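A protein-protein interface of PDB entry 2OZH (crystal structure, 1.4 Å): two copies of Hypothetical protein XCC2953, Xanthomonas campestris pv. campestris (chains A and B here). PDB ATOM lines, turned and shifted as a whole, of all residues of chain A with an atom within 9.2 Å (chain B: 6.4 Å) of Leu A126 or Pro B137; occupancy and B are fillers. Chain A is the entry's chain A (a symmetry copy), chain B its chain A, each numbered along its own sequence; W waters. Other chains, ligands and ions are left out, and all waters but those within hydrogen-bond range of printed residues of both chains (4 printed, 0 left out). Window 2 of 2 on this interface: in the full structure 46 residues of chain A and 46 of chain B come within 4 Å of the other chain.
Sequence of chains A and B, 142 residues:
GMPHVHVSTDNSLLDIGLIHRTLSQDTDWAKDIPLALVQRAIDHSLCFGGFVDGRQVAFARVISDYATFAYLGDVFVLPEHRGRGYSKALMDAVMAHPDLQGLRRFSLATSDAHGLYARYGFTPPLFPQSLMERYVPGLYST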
ATOM      1  N   LEU A 103      -6.581  13.359 -10.121  1.00  0.00           N
ATOM      2  CA  LEU A 103      -7.871  12.935  -9.649  1.00  0.00           C
ATOM      3  C   LEU A 103      -8.973  13.803 -10.213  1.00  0.00           C
ATOM      4  O   LEU A 103      -8.800  15.023 -10.327  1.00  0.00           O
ATOM      5  CB  LEU A 103      -7.902  13.032  -8.113  1.00  0.00           C
ATOM      6  CG  LEU A 103      -6.857  12.244  -7.329  1.00  0.00           C
ATOM      7  CD1 LEU A 103      -7.007  12.497  -5.847  1.00  0.00           C
ATOM      8  CD2 LEU A 103      -6.965  10.741  -7.601  1.00  0.00           C
ATOM      9  N   ARG A 104     -10.107  13.199 -10.503  1.00  0.00           N
ATOM     10  CA  ARG A 104     -11.273  13.917 -10.965  1.00  0.00           C
ATOM     11  C   ARG A 104     -11.859  14.780  -9.860  1.00  0.00           C
ATOM     12  O   ARG A 104     -12.286  15.922 -10.092  1.00  0.00           O
ATOM     13  CB  ARG A 104     -12.309  12.916 -11.449  1.00  0.00           C
ATOM     14  CG  ARG A 104     -13.389  13.572 -12.202  1.00  0.00           C
ATOM     15  CD  ARG A 104     -13.960  12.596 -13.186  1.00  0.00           C
ATOM     16  NE  ARG A 104     -15.110  13.255 -13.735  1.00  0.00           N
ATOM     17  CZ  ARG A 104     -16.247  13.374 -13.058  1.00  0.00           C
ATOM     18  NH1 ARG A 104     -16.380  12.822 -11.852  1.00  0.00           N
ATOM     19  NH2 ARG A 104     -17.249  14.014 -13.595  1.00  0.00           N
ATOM     20  N   ARG A 105     -11.903  14.228  -8.639  1.00  0.00           N
ATOM     21  CA  ARG A 105     -12.510  14.929  -7.512  1.00  0.00           C
ATOM     22  C   ARG A 105     -11.738  14.681  -6.234  1.00  0.00           C
ATOM     23  O   ARG A 105     -11.452  13.519  -5.889  1.00  0.00           O
ATOM     24  CB  ARG A 105     -13.948  14.465  -7.299  1.00  0.00           C
ATOM     25  CG  ARG A 105     -14.744  15.445  -6.412  1.00  0.00           C
ATOM     26  CD  ARG A 105     -16.070  14.909  -5.976  1.00  0.00           C
ATOM     27  NE  ARG A 105     -16.949  14.455  -7.045  1.00  0.00           N
ATOM     28  CZ  ARG A 105     -18.094  15.013  -7.434  1.00  0.00           C
ATOM     29  NH1 ARG A 105     -18.581  16.160  -6.950  1.00  0.00           N
ATOM     30  NH2 ARG A 105     -18.768  14.362  -8.345  1.00  0.00           N
ATOM     31  N   GLY A 121      -6.794  25.361  -3.962  1.00  0.00           N
ATOM     32  CA  GLY A 121      -7.609  25.118  -5.138  1.00  0.00           C
ATOM     33  C   GLY A 121      -8.999  24.553  -4.881  1.00  0.00           C
ATOM     34  O   GLY A 121      -9.772  24.354  -5.815  1.00  0.00           O
ATOM     35  N   PHE A 122      -9.351  24.317  -3.626  1.00  0.00           N
ATOM     36  CA  PHE A 122     -10.680  23.827  -3.299  1.00  0.00           C
ATOM     37  C   PHE A 122     -11.688  24.957  -3.479  1.00  0.00           C
ATOM     38  O   PHE A 122     -11.408  26.128  -3.177  1.00  0.00           O
ATOM     39  CB  PHE A 122     -10.720  23.261  -1.882  1.00  0.00           C
ATOM     40  CG  PHE A 122      -9.987  21.964  -1.724  1.00  0.00           C
ATOM     41  CD1 PHE A 122      -8.620  21.919  -1.469  1.00  0.00           C
ATOM     42  CD2 PHE A 122     -10.668  20.760  -1.809  1.00  0.00           C
ATOM     43  CE1 PHE A 122      -7.967  20.722  -1.350  1.00  0.00           C
ATOM     44  CE2 PHE A 122     -10.008  19.553  -1.676  1.00  0.00           C
ATOM     45  CZ  PHE A 122      -8.668  19.534  -1.446  1.00  0.00           C
ATOM     46  N   THR A 123     -12.873  24.601  -3.954  1.00  0.00           N
ATOM     47  CA  THR A 123     -13.956  25.539  -4.201  1.00  0.00           C
ATOM     48  C   THR A 123     -15.245  25.014  -3.582  1.00  0.00           C
ATOM     49  O   THR A 123     -15.371  23.818  -3.337  1.00  0.00           O
ATOM     50  CB  THR A 123     -14.209  25.726  -5.730  1.00  0.00           C
ATOM     51  OG1 THR A 123     -14.666  24.487  -6.299  1.00  0.00           O
ATOM     52  CG2 THR A 123     -12.957  26.173  -6.437  1.00  0.00           C
ATOM     53  N   PRO A 124     -16.262  25.872  -3.447  1.00  0.00           N
ATOM     54  CA  PRO A 124     -17.585  25.301  -3.187  1.00  0.00           C
ATOM     55  C   PRO A 124     -17.944  24.322  -4.313  1.00  0.00           C
ATOM     56  O   PRO A 124     -17.434  24.439  -5.426  1.00  0.00           O
ATOM     57  CB  PRO A 124     -18.514  26.523  -3.198  1.00  0.00           C
ATOM     58  CG  PRO A 124     -17.605  27.698  -2.952  1.00  0.00           C
ATOM     59  CD  PRO A 124     -16.276  27.339  -3.552  1.00  0.00           C
ATOM     60  N   PRO A 125     -18.836  23.367  -4.045  1.00  0.00           N
ATOM     61  CA  PRO A 125     -19.139  22.438  -5.105  1.00  0.00           C
ATOM     62  C   PRO A 125     -19.680  23.041  -6.351  1.00  0.00           C
ATOM     63  O   PRO A 125     -20.452  24.018  -6.325  1.00  0.00           O
ATOM     64  CB  PRO A 125     -20.165  21.507  -4.471  1.00  0.00           C
ATOM     65  CG  PRO A 125     -19.880  21.602  -2.992  1.00  0.00           C
ATOM     66  CD  PRO A 125     -19.578  23.045  -2.815  1.00  0.00           C
ATOM     67  N   LEU A 126     -19.281  22.459  -7.481  1.00  0.00           N
ATOM     68  CA  LEU A 126     -19.758  22.945  -8.748  1.00  0.00           C
ATOM     69  C   LEU A 126     -21.257  22.755  -8.888  1.00  0.00           C
ATOM     70  O   LEU A 126     -21.960  23.615  -9.474  1.00  0.00           O
ATOM     71  CB  LEU A 126     -19.056  22.244  -9.900  1.00  0.00           C
ATOM     72  CG  LEU A 126     -17.550  22.501  -9.970  1.00  0.00           C
ATOM     73  CD1 LEU A 126     -16.993  21.840 -11.228  1.00  0.00           C
ATOM     74  CD2 LEU A 126     -17.207  23.989  -9.925  1.00  0.00           C
ATOM     75  N   PHE A 127     -21.744  21.606  -8.438  1.00  0.00           N
ATOM     76  CA  PHE A 127     -23.098  21.137  -8.654  1.00  0.00           C
ATOM     77  C   PHE A 127     -23.709  20.696  -7.315  1.00  0.00           C
ATOM     78  O   PHE A 127     -23.919  19.504  -7.053  1.00  0.00           O
ATOM     79  CB  PHE A 127     -23.115  19.978  -9.652  1.00  0.00           C
ATOM     80  CG  PHE A 127     -22.228  20.191 -10.871  1.00  0.00           C
ATOM     81  CD1 PHE A 127     -22.299  21.339 -11.629  1.00  0.00           C
ATOM     82  CD2 PHE A 127     -21.316  19.224 -11.240  1.00  0.00           C
ATOM     83  CE1 PHE A 127     -21.469  21.536 -12.739  1.00  0.00           C
ATOM     84  CE2 PHE A 127     -20.481  19.412 -12.342  1.00  0.00           C
ATOM     85  CZ  PHE A 127     -20.548  20.559 -13.080  1.00  0.00           C
ATOM     86  N   PRO A 128     -23.984  21.664  -6.435  1.00  0.00           N
ATOM     87  CA  PRO A 128     -24.362  21.296  -5.068  1.00  0.00           C
ATOM     88  C   PRO A 128     -25.623  20.464  -4.997  1.00  0.00           C
ATOM     89  O   PRO A 128     -25.764  19.637  -4.062  1.00  0.00           O
ATOM     90  CB  PRO A 128     -24.533  22.665  -4.371  1.00  0.00           C
ATOM     91  CG  PRO A 128     -24.705  23.644  -5.475  1.00  0.00           C
ATOM     92  CD  PRO A 128     -23.889  23.119  -6.603  1.00  0.00           C
ATOM     93  N   GLN A 129     -26.562  20.644  -5.924  1.00  0.00           N
ATOM     94  CA  GLN A 129     -27.798  19.881  -5.894  1.00  0.00           C
ATOM     95  C   GLN A 129     -27.587  18.408  -6.182  1.00  0.00           C
ATOM     96  O   GLN A 129     -28.462  17.594  -5.898  1.00  0.00           O
ATOM     97  CB  GLN A 129     -28.804  20.481  -6.890  1.00  0.00           C
ATOM     98  CG  GLN A 129     -30.215  19.891  -6.842  1.00  0.00           C
ATOM     99  CD  GLN A 129     -30.500  18.762  -7.857  1.00  0.00           C
ATOM    100  OE1 GLN A 129     -29.659  18.398  -8.687  1.00  0.00           O
ATOM    101  NE2 GLN A 129     -31.700  18.193  -7.766  1.00  0.00           N
ATOM    102  N   SER A 130     -26.449  18.040  -6.772  1.00  0.00           N
ATOM    103  CA  SER A 130     -26.155  16.646  -7.042  1.00  0.00           C
ATOM    104  C   SER A 130     -25.730  15.848  -5.820  1.00  0.00           C
ATOM    105  O   SER A 130     -25.710  14.611  -5.841  1.00  0.00           O
ATOM    106  CB  SER A 130     -25.025  16.518  -8.070  1.00  0.00           C
ATOM    107  OG  SER A 130     -23.752  16.941  -7.559  1.00  0.00           O
ATOM    108  N   LEU A 131     -25.309  16.541  -4.770  1.00  0.00           N
ATOM    109  CA  LEU A 131     -24.675  15.871  -3.650  1.00  0.00           C
ATOM    110  C   LEU A 131     -25.700  15.286  -2.687  1.00  0.00           C
ATOM    111  O   LEU A 131     -26.710  15.912  -2.333  1.00  0.00           O
ATOM    112  CB  LEU A 131     -23.788  16.868  -2.925  1.00  0.00           C
ATOM    113  CG  LEU A 131     -22.738  17.522  -3.823  1.00  0.00           C
ATOM    114  CD1 LEU A 131     -21.842  18.448  -2.986  1.00  0.00           C
ATOM    115  CD2 LEU A 131     -21.896  16.505  -4.566  1.00  0.00           C
ATOM    116  N   GLU B 133     -14.483  21.150  -2.843  1.00  0.00           N
ATOM    117  CA  GLU B 133     -13.851  20.185  -3.709  1.00  0.00           C
ATOM    118  C   GLU B 133     -12.896  20.812  -4.708  1.00  0.00           C
ATOM    119  O   GLU B 133     -13.032  21.992  -5.068  1.00  0.00           O
ATOM    120  CB  GLU B 133     -14.901  19.377  -4.472  1.00  0.00           C
ATOM    121  CG  GLU B 133     -15.848  20.218  -5.315  1.00  0.00           C
ATOM    122  CD  GLU B 133     -17.003  19.423  -5.952  1.00  0.00           C
ATOM    123  OE1 GLU B 133     -17.208  18.223  -5.636  1.00  0.00           O
ATOM    124  OE2 GLU B 133     -17.711  20.025  -6.784  1.00  0.00           O
ATOM    125  N   TYR B 135     -12.684  19.792  -8.270  1.00  0.00           N
ATOM    126  CA  TYR B 135     -13.447  18.943  -9.168  1.00  0.00           C
ATOM    127  C   TYR B 135     -13.286  19.402 -10.598  1.00  0.00           C
ATOM    128  O   TYR B 135     -13.559  20.557 -10.892  1.00  0.00           O
ATOM    129  CB  TYR B 135     -14.916  18.946  -8.753  1.00  0.00           C
ATOM    130  CG  TYR B 135     -15.861  18.047  -9.524  1.00  0.00           C
ATOM    131  CD1 TYR B 135     -15.446  16.866 -10.052  1.00  0.00           C
ATOM    132  CD2 TYR B 135     -17.203  18.360  -9.624  1.00  0.00           C
ATOM    133  CE1 TYR B 135     -16.304  16.027 -10.727  1.00  0.00           C
ATOM    134  CE2 TYR B 135     -18.091  17.506 -10.300  1.00  0.00           C
ATOM    135  CZ  TYR B 135     -17.629  16.359 -10.838  1.00  0.00           C
ATOM    136  OH  TYR B 135     -18.461  15.475 -11.522  1.00  0.00           O
ATOM    137  N   VAL B 136     -12.811  18.501 -11.455  1.00  0.00           N
ATOM    138  CA  VAL B 136     -12.552  18.785 -12.878  1.00  0.00           C
ATOM    139  C   VAL B 136     -13.398  17.828 -13.686  1.00  0.00           C
ATOM    140  O   VAL B 136     -12.913  16.794 -14.161  1.00  0.00           O
ATOM    141  CB  VAL B 136     -11.068  18.656 -13.204  1.00  0.00           C
ATOM    142  CG1 VAL B 136     -10.797  19.060 -14.657  1.00  0.00           C
ATOM    143  CG2 VAL B 136     -10.249  19.552 -12.267  1.00  0.00           C
ATOM    144  N   PRO B 137     -14.693  18.140 -13.851  1.00  0.00           N
ATOM    145  CA  PRO B 137     -15.508  17.347 -14.772  1.00  0.00           C
ATOM    146  C   PRO B 137     -14.942  17.410 -16.186  1.00  0.00           C
ATOM    147  O   PRO B 137     -14.476  18.451 -16.618  1.00  0.00           O
ATOM    148  CB  PRO B 137     -16.897  18.011 -14.693  1.00  0.00           C
ATOM    149  CG  PRO B 137     -16.688  19.308 -14.078  1.00  0.00           C
ATOM    150  CD  PRO B 137     -15.485  19.189 -13.188  1.00  0.00           C
ATOM    151  N   GLY B 138     -14.941  16.288 -16.893  1.00  0.00           N
ATOM    152  CA  GLY B 138     -14.368  16.258 -18.242  1.00  0.00           C
ATOM    153  C   GLY B 138     -12.843  16.255 -18.272  1.00  0.00           C
ATOM    154  O   GLY B 138     -12.232  16.539 -19.307  1.00  0.00           O
ATOM    155  N   LEU B 139     -12.209  15.898 -17.152  1.00  0.00           N
ATOM    156  CA  LEU B 139     -10.742  15.758 -17.090  1.00  0.00           C
ATOM    157  C   LEU B 139     -10.126  14.853 -18.164  1.00  0.00           C
ATOM    158  O   LEU B 139      -9.034  15.092 -18.641  1.00  0.00           O
ATOM    159  CB  LEU B 139     -10.343  15.185 -15.715  1.00  0.00           C
ATOM    160  CG  LEU B 139      -8.856  14.951 -15.418  1.00  0.00           C
ATOM    161  CD1 LEU B 139      -8.052  16.203 -15.586  1.00  0.00           C
ATOM    162  CD2 LEU B 139      -8.714  14.439 -14.013  1.00  0.00           C
ATOM    163  N   TYR B 140     -10.798  13.742 -18.465  1.00  0.00           N
ATOM    164  CA  TYR B 140     -10.191  12.729 -19.337  1.00  0.00           C
ATOM    165  C   TYR B 140     -10.323  13.041 -20.820  1.00  0.00           C
ATOM    166  O   TYR B 140      -9.708  12.369 -21.641  1.00  0.00           O
ATOM    167  CB  TYR B 140     -10.796  11.329 -19.093  1.00  0.00           C
ATOM    168  CG  TYR B 140     -10.852  10.951 -17.634  1.00  0.00           C
ATOM    169  CD1 TYR B 140      -9.721  10.997 -16.835  1.00  0.00           C
ATOM    170  CD2 TYR B 140     -12.051  10.555 -17.055  1.00  0.00           C
ATOM    171  CE1 TYR B 140      -9.792  10.668 -15.512  1.00  0.00           C
ATOM    172  CE2 TYR B 140     -12.127  10.226 -15.719  1.00  0.00           C
ATOM    173  CZ  TYR B 140     -11.006  10.299 -14.964  1.00  0.00           C
ATOM    174  OH  TYR B 140     -11.098   9.996 -13.621  1.00  0.00           O
HETATM  175  O   HOH W   1     -15.536  13.318 -16.610  1.00  0.00           O
HETATM  176  O   HOH W   2     -20.237  19.393  -7.480  1.00  0.00           O
HETATM  177  O   HOH W   3      -9.040  10.752 -12.154  1.00  0.00           O
HETATM  178  O   HOH W   4     -13.222  22.658  -8.093  1.00  0.00           O
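The side-chain carboxylate of Glu B133 lies within salt-bridge range of the guanidinium group of Arg A105. The backbone NH (N) of Thr A123 lies within hydrogen-bond range of the backbone carbonyl oxygen (O) of Glu B133 (2.8 Å). OE2 of Glu B133 sits at hydrogen-bond distance from N of Leu A126. NH2 of Arg A104 lies within hydrogen-bond range of OH of Tyr B135 (2.8 Å). The side-chain hydroxyl of Tyr B135 lies within hydrogen-bond range of the guanidinium group of Arg A105 (3.4 Å). N of Val B136 is in hydrogen-bond range of O of Arg A104 (3.0 Å).
O of Phe A127 lies within hydrogen-bond range of OG of Ser A130.
Leu B139 touches Leu A103. NH2 of Arg A104 touches CA of Pro B137, 3.9 Å away. Arg A104 touches Leu B139 (N to CD2, 3.97 Å). Tyr B140 touches Arg A104. Glu B133 touches Phe A122. Pro A125 touches Glu B133 (CA to OE2, 3.3 Å). CD1 of Leu A126 touches O of Tyr B135, at 3.7 Å. Pro B137 touches Leu A126. CE2 of Phe A127 touches CE2 of Tyr B135, 3.7 Å away.
Printed residues of chain A within 4 Å of Pro B137: Arg A104 and Leu A126. Of the printed residues of chain B, Pro A125 touches Glu B133. Printed residues of chain A within 4 Å of Val B136: Arg A104. The nearest printed residue of chain B that does not touch Leu A126 is Val B136 (5.4 Å). The nearest printed residue of chain A that does not touch Pro B137 is Phe A127 (4.2 Å).
Of the 14 printed residues of chain A, 8 touch a printed residue of chain B. Hydrophobic or aromatic side chains of chain A within 4 Å of the printed part of chain B: Phe A122, Pro A125, Leu A126 and Phe A127. Hydrophobic or aromatic side chains of chain B that line the printed part of chain A: Tyr B135, Pro B137, Leu B139 and Tyr B140.
No position is printed for both chains. Of the 15 pairs that touch across the chains among the printed residues, none has its exchanged pair printed and touching as well.
Water W3 bridges the side-chain hydroxyl (OH) of Tyr B140 (2.6 Å) and the backbone NH (N) of Arg A104 (3.1 Å). Water W2 lies within hydrogen-bond range of OE2 of Glu B133, N of Phe A127 and N of Leu A126. Water W1 lies within hydrogen-bond range of NE of Arg A104 (2.9 Å) and N of Gly B138 (3.0 Å). Water W4 lies within hydrogen-bond range of N of Tyr B135, OG1 of Thr A123 and O of Glu B133.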
